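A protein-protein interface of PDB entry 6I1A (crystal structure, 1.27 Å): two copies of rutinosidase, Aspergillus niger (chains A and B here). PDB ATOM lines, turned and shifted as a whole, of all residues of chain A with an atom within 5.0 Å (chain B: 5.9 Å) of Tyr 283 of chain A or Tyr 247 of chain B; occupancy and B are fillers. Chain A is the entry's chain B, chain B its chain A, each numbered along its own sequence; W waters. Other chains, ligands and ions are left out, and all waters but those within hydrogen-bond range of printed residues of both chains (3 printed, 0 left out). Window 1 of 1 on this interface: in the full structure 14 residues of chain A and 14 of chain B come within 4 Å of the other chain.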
ATOM      1  N   TYR A 269     -18.444 -17.139 -34.090  1.00  0.00           N
ATOM      2  CA  TYR A 269     -18.521 -16.082 -33.096  1.00  0.00           C
ATOM      3  C   TYR A 269     -17.160 -15.521 -32.746  1.00  0.00           C
ATOM      4  O   TYR A 269     -17.094 -14.693 -31.815  1.00  0.00           O
ATOM      5  CB  TYR A 269     -19.190 -16.645 -31.847  1.00  0.00           C
ATOM      6  CG  TYR A 269     -20.522 -17.298 -32.151  1.00  0.00           C
ATOM      7  CD1 TYR A 269     -21.656 -16.546 -32.386  1.00  0.00           C
ATOM      8  CD2 TYR A 269     -20.602 -18.671 -32.315  1.00  0.00           C
ATOM      9  CE1 TYR A 269     -22.839 -17.142 -32.791  1.00  0.00           C
ATOM     10  CE2 TYR A 269     -21.768 -19.273 -32.698  1.00  0.00           C
ATOM     11  CZ  TYR A 269     -22.870 -18.502 -32.998  1.00  0.00           C
ATOM     12  OH  TYR A 269     -24.031 -19.076 -33.442  1.00  0.00           O
ATOM     13  N   MET A 273     -17.690  -9.235 -33.265  1.00  0.00           N
ATOM     14  CA  MET A 273     -18.887  -9.096 -32.434  1.00  0.00           C
ATOM     15  C   MET A 273     -18.461  -9.116 -30.957  1.00  0.00           C
ATOM     16  O   MET A 273     -17.363  -9.525 -30.611  1.00  0.00           O
ATOM     17  CB  MET A 273     -19.890 -10.221 -32.739  1.00  0.00           C
ATOM     18  CG  MET A 273     -19.355 -11.578 -32.414  1.00  0.00           C
ATOM     19  SD  MET A 273     -20.537 -12.898 -32.913  1.00  0.00           S
ATOM     20  CE  MET A 273     -20.148 -12.981 -34.632  1.00  0.00           C
ATOM     21  N   ASP A 274     -19.369  -8.663 -30.103  1.00  0.00           N
ATOM     22  CA  ASP A 274     -19.096  -8.569 -28.650  1.00  0.00           C
ATOM     23  C   ASP A 274     -19.506  -9.878 -27.959  1.00  0.00           C
ATOM     24  O   ASP A 274     -20.101  -9.876 -26.867  1.00  0.00           O
ATOM     25  CB  ASP A 274     -19.830  -7.367 -28.050  1.00  0.00           C
ATOM     26  CG  ASP A 274     -19.266  -6.069 -28.604  1.00  0.00           C
ATOM     27  OD1 ASP A 274     -18.031  -5.964 -28.686  1.00  0.00           O
ATOM     28  OD2 ASP A 274     -20.061  -5.179 -28.938  1.00  0.00           O
ATOM     29  N   SER A 275     -19.159 -11.001 -28.566  1.00  0.00           N
ATOM     30  CA  SER A 275     -19.411 -12.320 -27.955  1.00  0.00           C
ATOM     31  C   SER A 275     -18.347 -12.614 -26.886  1.00  0.00           C
ATOM     32  O   SER A 275     -17.171 -12.271 -27.038  1.00  0.00           O
ATOM     33  CB  SER A 275     -19.439 -13.405 -29.005  1.00  0.00           C
ATOM     34  OG  SER A 275     -18.221 -13.427 -29.733  1.00  0.00           O
ATOM     35  N   ASN A 279     -21.837 -15.042 -22.724  1.00  0.00           N
ATOM     36  CA  ASN A 279     -23.052 -14.666 -23.470  1.00  0.00           C
ATOM     37  C   ASN A 279     -23.260 -15.465 -24.748  1.00  0.00           C
ATOM     38  O   ASN A 279     -24.262 -15.246 -25.466  1.00  0.00           O
ATOM     39  CB  ASN A 279     -23.021 -13.161 -23.721  1.00  0.00           C
ATOM     40  CG  ASN A 279     -22.040 -12.702 -24.767  1.00  0.00           C
ATOM     41  OD1 ASN A 279     -21.605 -13.505 -25.622  1.00  0.00           O
ATOM     42  ND2 ASN A 279     -21.701 -11.433 -24.730  1.00  0.00           N
ATOM     43  N   LEU A 280     -22.415 -16.455 -24.982  1.00  0.00           N
ATOM     44  CA  LEU A 280     -22.455 -17.156 -26.291  1.00  0.00           C
ATOM     45  C   LEU A 280     -23.820 -17.739 -26.557  1.00  0.00           C
ATOM     46  O   LEU A 280     -24.285 -17.676 -27.708  1.00  0.00           O
ATOM     47  CB  LEU A 280     -21.400 -18.275 -26.331  1.00  0.00           C
ATOM     48  CG  LEU A 280     -21.130 -18.763 -27.756  1.00  0.00           C
ATOM     49  CD1 LEU A 280     -20.259 -17.766 -28.511  1.00  0.00           C
ATOM     50  CD2 LEU A 280     -20.468 -20.119 -27.737  1.00  0.00           C
ATOM     51  N   PRO A 281     -24.536 -18.350 -25.571  1.00  0.00           N
ATOM     52  CA  PRO A 281     -25.862 -18.873 -25.900  1.00  0.00           C
ATOM     53  C   PRO A 281     -26.859 -17.866 -26.460  1.00  0.00           C
ATOM     54  O   PRO A 281     -27.728 -18.274 -27.241  1.00  0.00           O
ATOM     55  CB  PRO A 281     -26.337 -19.498 -24.579  1.00  0.00           C
ATOM     56  CG  PRO A 281     -25.043 -19.822 -23.878  1.00  0.00           C
ATOM     57  CD  PRO A 281     -24.144 -18.648 -24.178  1.00  0.00           C
ATOM     58  N   GLU A 282     -26.716 -16.604 -26.091  1.00  0.00           N
ATOM     59  CA  GLU A 282     -27.567 -15.500 -26.647  1.00  0.00           C
ATOM     60  C   GLU A 282     -27.262 -15.295 -28.112  1.00  0.00           C
ATOM     61  O   GLU A 282     -28.204 -15.119 -28.934  1.00  0.00           O
ATOM     62  CB  GLU A 282     -27.372 -14.182 -25.902  1.00  0.00           C
ATOM     63  CG  GLU A 282     -27.717 -14.302 -24.441  1.00  0.00           C
ATOM     64  CD  GLU A 282     -27.191 -13.186 -23.541  1.00  0.00           C
ATOM     65  OE1 GLU A 282     -26.917 -12.090 -24.042  1.00  0.00           O
ATOM     66  OE2 GLU A 282     -26.865 -13.513 -22.362  1.00  0.00           O
ATOM     67  N   TYR A 283     -25.991 -15.346 -28.528  1.00  0.00           N
ATOM     68  CA  TYR A 283     -25.610 -15.181 -29.940  1.00  0.00           C
ATOM     69  C   TYR A 283     -26.036 -16.402 -30.755  1.00  0.00           C
ATOM     70  O   TYR A 283     -26.528 -16.258 -31.894  1.00  0.00           O
ATOM     71  CB  TYR A 283     -24.089 -14.960 -30.031  1.00  0.00           C
ATOM     72  CG  TYR A 283     -23.686 -13.534 -29.725  1.00  0.00           C
ATOM     73  CD1 TYR A 283     -23.606 -12.581 -30.734  1.00  0.00           C
ATOM     74  CD2 TYR A 283     -23.338 -13.151 -28.433  1.00  0.00           C
ATOM     75  CE1 TYR A 283     -23.248 -11.271 -30.489  1.00  0.00           C
ATOM     76  CE2 TYR A 283     -23.051 -11.823 -28.172  1.00  0.00           C
ATOM     77  CZ  TYR A 283     -22.976 -10.903 -29.189  1.00  0.00           C
ATOM     78  OH  TYR A 283     -22.670  -9.571 -28.920  1.00  0.00           O
ATOM     79  N   ILE A 284     -25.926 -17.597 -30.185  1.00  0.00           N
ATOM     80  CA  ILE A 284     -26.379 -18.839 -30.857  1.00  0.00           C
ATOM     81  C   ILE A 284     -27.905 -18.791 -31.052  1.00  0.00           C
ATOM     82  O   ILE A 284     -28.397 -19.054 -32.160  1.00  0.00           O
ATOM     83  CB  ILE A 284     -25.937 -20.039 -30.013  1.00  0.00           C
ATOM     84  CG1 ILE A 284     -24.419 -20.255 -30.090  1.00  0.00           C
ATOM     85  CG2 ILE A 284     -26.682 -21.293 -30.452  1.00  0.00           C
ATOM     86  CD1 ILE A 284     -23.927 -21.241 -29.057  1.00  0.00           C
ATOM     87  N   LEU A 285     -28.649 -18.401 -30.007  1.00  0.00           N
ATOM     88  CA  LEU A 285     -30.142 -18.264 -30.132  1.00  0.00           C
ATOM     89  C   LEU A 285     -30.486 -17.243 -31.205  1.00  0.00           C
ATOM     90  O   LEU A 285     -31.359 -17.480 -32.043  1.00  0.00           O
ATOM     91  CB  LEU A 285     -30.719 -17.905 -28.780  1.00  0.00           C
ATOM     92  CG  LEU A 285     -32.242 -17.688 -28.824  1.00  0.00           C
ATOM     93  CD1 LEU A 285     -32.974 -18.910 -29.318  1.00  0.00           C
ATOM     94  CD2 LEU A 285     -32.664 -17.229 -27.416  1.00  0.00           C
ATOM     95  N   ALA A 286     -29.803 -16.104 -31.231  1.00  0.00           N
ATOM     96  CA  ALA A 286     -30.060 -15.073 -32.240  1.00  0.00           C
ATOM     97  C   ALA A 286     -29.894 -15.638 -33.633  1.00  0.00           C
ATOM     98  O   ALA A 286     -30.717 -15.431 -34.547  1.00  0.00           O
ATOM     99  CB  ALA A 286     -29.200 -13.844 -32.022  1.00  0.00           C
ATOM    100  N   ASP A 287     -28.791 -16.349 -33.886  1.00  0.00           N
ATOM    101  CA  ASP A 287     -28.578 -16.919 -35.211  1.00  0.00           C
ATOM    102  C   ASP A 287     -29.669 -17.949 -35.558  1.00  0.00           C
ATOM    103  O   ASP A 287     -30.178 -17.960 -36.710  1.00  0.00           O
ATOM    104  CB  ASP A 287     -27.232 -17.626 -35.246  1.00  0.00           C
ATOM    105  CG  ASP A 287     -26.039 -16.699 -35.362  1.00  0.00           C
ATOM    106  OD1 ASP A 287     -26.228 -15.510 -35.751  1.00  0.00           O
ATOM    107  OD2 ASP A 287     -24.900 -17.181 -35.127  1.00  0.00           O
ATOM    108  N   PRO B 208     -22.212  -3.044 -34.034  1.00  0.00           N
ATOM    109  CA  PRO B 208     -21.342  -2.963 -32.850  1.00  0.00           C
ATOM    110  C   PRO B 208     -19.893  -2.602 -33.180  1.00  0.00           C
ATOM    111  O   PRO B 208     -19.185  -2.150 -32.277  1.00  0.00           O
ATOM    112  CB  PRO B 208     -21.437  -4.371 -32.261  1.00  0.00           C
ATOM    113  CG  PRO B 208     -22.877  -4.773 -32.608  1.00  0.00           C
ATOM    114  CD  PRO B 208     -23.041  -4.280 -34.014  1.00  0.00           C
ATOM    115  N   GLY B 243     -26.587   4.005 -26.577  1.00  0.00           N
ATOM    116  CA  GLY B 243     -25.304   3.306 -26.494  1.00  0.00           C
ATOM    117  C   GLY B 243     -24.794   2.862 -27.839  1.00  0.00           C
ATOM    118  O   GLY B 243     -24.379   1.711 -28.014  1.00  0.00           O
ATOM    119  N   PHE B 245     -24.497   1.394 -31.387  1.00  0.00           N
ATOM    120  CA  PHE B 245     -25.184   0.247 -32.014  1.00  0.00           C
ATOM    121  C   PHE B 245     -24.749  -1.011 -31.322  1.00  0.00           C
ATOM    122  O   PHE B 245     -24.929  -2.092 -31.894  1.00  0.00           O
ATOM    123  CB  PHE B 245     -24.929   0.235 -33.521  1.00  0.00           C
ATOM    124  CG  PHE B 245     -25.246   1.545 -34.190  1.00  0.00           C
ATOM    125  CD1 PHE B 245     -26.575   1.910 -34.427  1.00  0.00           C
ATOM    126  CD2 PHE B 245     -24.243   2.425 -34.496  1.00  0.00           C
ATOM    127  CE1 PHE B 245     -26.840   3.159 -35.009  1.00  0.00           C
ATOM    128  CE2 PHE B 245     -24.498   3.651 -35.061  1.00  0.00           C
ATOM    129  CZ  PHE B 245     -25.787   4.018 -35.309  1.00  0.00           C
ATOM    130  N   LYS B 246     -24.265  -0.938 -30.083  1.00  0.00           N
ATOM    131  CA  LYS B 246     -24.060  -2.137 -29.244  1.00  0.00           C
ATOM    132  C   LYS B 246     -25.424  -2.679 -28.843  1.00  0.00           C
ATOM    133  O   LYS B 246     -26.423  -1.896 -28.667  1.00  0.00           O
ATOM    134  CB  LYS B 246     -23.316  -1.758 -27.956  1.00  0.00           C
ATOM    135  CG  LYS B 246     -22.004  -1.141 -28.201  1.00  0.00           C
ATOM    136  CD  LYS B 246     -21.060  -1.991 -28.927  1.00  0.00           C
ATOM    137  CE  LYS B 246     -19.603  -1.796 -28.610  1.00  0.00           C
ATOM    138  NZ  LYS B 246     -18.778  -2.726 -29.446  1.00  0.00           N
ATOM    139  N   TYR B 247     -25.514  -3.969 -28.658  1.00  0.00           N
ATOM    140  CA  TYR B 247     -26.741  -4.525 -28.030  1.00  0.00           C
ATOM    141  C   TYR B 247     -26.865  -3.958 -26.625  1.00  0.00           C
ATOM    142  O   TYR B 247     -25.857  -3.727 -25.971  1.00  0.00           O
ATOM    143  CB  TYR B 247     -26.610  -6.030 -28.100  1.00  0.00           C
ATOM    144  CG  TYR B 247     -26.505  -6.448 -29.549  1.00  0.00           C
ATOM    145  CD1 TYR B 247     -26.970  -5.607 -30.580  1.00  0.00           C
ATOM    146  CD2 TYR B 247     -25.718  -7.494 -29.904  1.00  0.00           C
ATOM    147  CE1 TYR B 247     -26.769  -5.922 -31.927  1.00  0.00           C
ATOM    148  CE2 TYR B 247     -25.562  -7.858 -31.233  1.00  0.00           C
ATOM    149  CZ  TYR B 247     -26.087  -7.087 -32.248  1.00  0.00           C
ATOM    150  OH  TYR B 247     -25.804  -7.444 -33.549  1.00  0.00           O
ATOM    151  N   PRO B 248     -28.095  -3.654 -26.118  1.00  0.00           N
ATOM    152  CA  PRO B 248     -28.245  -3.145 -24.766  1.00  0.00           C
ATOM    153  C   PRO B 248     -27.526  -4.033 -23.761  1.00  0.00           C
ATOM    154  O   PRO B 248     -27.003  -3.511 -22.776  1.00  0.00           O
ATOM    155  CB  PRO B 248     -29.774  -3.118 -24.546  1.00  0.00           C
ATOM    156  CG  PRO B 248     -30.329  -2.936 -25.960  1.00  0.00           C
ATOM    157  CD  PRO B 248     -29.385  -3.701 -26.838  1.00  0.00           C
ATOM    158  N   GLN B 249     -27.531  -5.363 -23.967  1.00  0.00           N
ATOM    159  CA  GLN B 249     -26.846  -6.328 -23.101  1.00  0.00           C
ATOM    160  C   GLN B 249     -25.393  -5.933 -22.850  1.00  0.00           C
ATOM    161  O   GLN B 249     -24.820  -6.232 -21.800  1.00  0.00           O
ATOM    162  CB  GLN B 249     -26.865  -7.738 -23.739  1.00  0.00           C
ATOM    163  CG  GLN B 249     -28.194  -8.180 -24.387  1.00  0.00           C
ATOM    164  CD  GLN B 249     -28.631  -7.693 -25.749  1.00  0.00           C
ATOM    165  OE1 GLN B 249     -29.356  -6.716 -25.896  1.00  0.00           O
ATOM    166  NE2 GLN B 249     -28.503  -8.519 -26.801  1.00  0.00           N
ATOM    167  N   TYR B 250     -24.735  -5.277 -23.825  1.00  0.00           N
ATOM    168  CA  TYR B 250     -23.338  -4.858 -23.708  1.00  0.00           C
ATOM    169  C   TYR B 250     -23.165  -3.926 -22.534  1.00  0.00           C
ATOM    170  O   TYR B 250     -22.085  -3.932 -21.892  1.00  0.00           O
ATOM    171  CB  TYR B 250     -22.864  -4.176 -24.995  1.00  0.00           C
ATOM    172  CG  TYR B 250     -21.462  -3.657 -24.994  1.00  0.00           C
ATOM    173  CD1 TYR B 250     -20.414  -4.435 -25.424  1.00  0.00           C
ATOM    174  CD2 TYR B 250     -21.166  -2.326 -24.662  1.00  0.00           C
ATOM    175  CE1 TYR B 250     -19.117  -3.957 -25.423  1.00  0.00           C
ATOM    176  CE2 TYR B 250     -19.897  -1.829 -24.715  1.00  0.00           C
ATOM    177  CZ  TYR B 250     -18.855  -2.656 -25.044  1.00  0.00           C
ATOM    178  OH  TYR B 250     -17.624  -2.113 -25.096  1.00  0.00           O
ATOM    179  N   TRP B 251     -24.145  -3.047 -22.301  1.00  0.00           N
ATOM    180  CA  TRP B 251     -24.014  -1.975 -21.298  1.00  0.00           C
ATOM    181  C   TRP B 251     -24.700  -2.327 -19.971  1.00  0.00           C
ATOM    182  O   TRP B 251     -24.495  -1.642 -18.996  1.00  0.00           O
ATOM    183  CB  TRP B 251     -24.657  -0.669 -21.819  1.00  0.00           C
ATOM    184  CG  TRP B 251     -24.137  -0.163 -23.125  1.00  0.00           C
ATOM    185  CD1 TRP B 251     -24.741  -0.209 -24.343  1.00  0.00           C
ATOM    186  CD2 TRP B 251     -22.951   0.623 -23.312  1.00  0.00           C
ATOM    187  NE1 TRP B 251     -23.966   0.431 -25.290  1.00  0.00           N
ATOM    188  CE2 TRP B 251     -22.878   0.971 -24.674  1.00  0.00           C
ATOM    189  CE3 TRP B 251     -21.916   0.987 -22.437  1.00  0.00           C
ATOM    190  CZ2 TRP B 251     -21.828   1.718 -25.186  1.00  0.00           C
ATOM    191  CZ3 TRP B 251     -20.890   1.739 -22.961  1.00  0.00           C
ATOM    192  CH2 TRP B 251     -20.843   2.101 -24.302  1.00  0.00           C
ATOM    193  N   GLU B 290     -33.815  -9.629 -30.770  1.00  0.00           N
ATOM    194  CA  GLU B 290     -32.395  -9.842 -30.379  1.00  0.00           C
ATOM    195  C   GLU B 290     -31.773  -8.583 -29.806  1.00  0.00           C
ATOM    196  O   GLU B 290     -30.642  -8.721 -29.240  1.00  0.00           O
ATOM    197  CB  GLU B 290     -31.577 -10.301 -31.582  1.00  0.00           C
ATOM    198  CG  GLU B 290     -32.219 -11.390 -32.402  1.00  0.00           C
ATOM    199  CD  GLU B 290     -32.635 -12.647 -31.660  1.00  0.00           C
ATOM    200  OE1 GLU B 290     -32.193 -12.903 -30.511  1.00  0.00           O
ATOM    201  OE2 GLU B 290     -33.473 -13.430 -32.231  1.00  0.00           O
ATOM    202  N   LYS B 291     -32.370  -7.396 -29.949  1.00  0.00           N
ATOM    203  CA  LYS B 291     -31.681  -6.129 -29.618  1.00  0.00           C
ATOM    204  C   LYS B 291     -32.514  -5.335 -28.611  1.00  0.00           C
ATOM    205  O   LYS B 291     -32.472  -4.074 -28.698  1.00  0.00           O
ATOM    206  CB  LYS B 291     -31.386  -5.312 -30.887  1.00  0.00           C
ATOM    207  CG  LYS B 291     -30.622  -6.101 -31.937  1.00  0.00           C
ATOM    208  CD  LYS B 291     -30.403  -5.337 -33.249  1.00  0.00           C
ATOM    209  CE  LYS B 291     -29.791  -6.211 -34.307  1.00  0.00           C
ATOM    210  NZ  LYS B 291     -29.651  -5.560 -35.637  1.00  0.00           N
HETATM  211  O   HOH W   1     -16.499  -3.771 -28.107  1.00  0.00           O
HETATM  212  O   HOH W   2     -30.624 -13.748 -28.257  1.00  0.00           O
HETATM  213  O   HOH W   3     -22.822  -5.543 -28.930  1.00  0.00           O
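Of the 13 printed residues of chain A, 3 touch a printed residue of chain B.
Hydrophobic or aromatic side chains of chain A within 4 Å of the printed part of chain B: Tyr 283 and Ala 286.
Of the 11 printed residues of chain B, 5 touch a printed residue of chain A.
Among the printed residues, Asp or Glu carboxylates within 4 Å of a Lys or Arg side-chain nitrogen of the other chain: Asp 274 of chain A with Lys 246 of chain B (2.8 Å).
Of chain B, only Tyr 247 (3.8 Å) comes within 4 Å of Tyr 283 of chain A.
Tyr 247 of chain B touches one residue of chain A.
Printed residues of chain A within 4 Å of Lys 246 of chain B: Asp 274.
Of the printed residues of chain A, Tyr 250 of chain B touches Asp 274 (3.6 Å).
The nearest printed residue of chain B that does not touch Ala 286 of chain A is Tyr 247 of chain B (7.0 Å).
No position is printed for both chains.
Of the 5 pairs that touch across the chains among the printed residues, none has its exchanged pair printed and touching as well.
The side-chain amino group of Lys 246 of chain B is in salt-bridge range of the side-chain carboxylate of Asp 274 of chain A, 2.8 Å away.
Among the printed residues, merely in contact across the chains: Asp 274 of chain A with Pro 208 of chain B (3.7 Å), Asp 274 of chain A with Tyr 250 of chain B (3.6 Å), Tyr 283 of chain A with Tyr 247 of chain B (3.8 Å) and Ala 286 of chain A with Glu 290 of chain B (3.5 Å).
Water W1 bridges the side-chain carboxylate (OD1) of Asp 274 of chain A (2.7 Å) and the side-chain amino group (NZ) of Lys 246 of chain B (2.8 Å).
Water W3 bridges OD2 of Asp 274 of chain A (2.8 Å) and N of Tyr 247 of chain B (3.1 Å).
Water W2 bridges the backbone carbonyl oxygen (O) of Glu 282 of chain A (2.9 Å) and the side-chain carboxylate (OE1) of Glu 290 of chain B (2.9 Å).
O of Glu 290 of chain B sits at hydrogen-bond distance from NE2 of Gln 249 of chain B, 3.3 Å away.
The backbone carbonyl oxygen (O) of Pro 208 of chain B sits at hydrogen-bond distance from the side-chain amino group (NZ) of Lys 246 of chain B.
The backbone carbonyl oxygen (O) of Asp 274 of chain A lies within hydrogen-bond range of the side-chain hydroxyl (OH) of Tyr 283 of chain A, 3.3 Å away.
The side-chain amide nitrogen (ND2) of Asn 279 of chain A sits at hydrogen-bond distance from the backbone carbonyl oxygen (O) of Asp 274 of chain A (3.1 Å).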
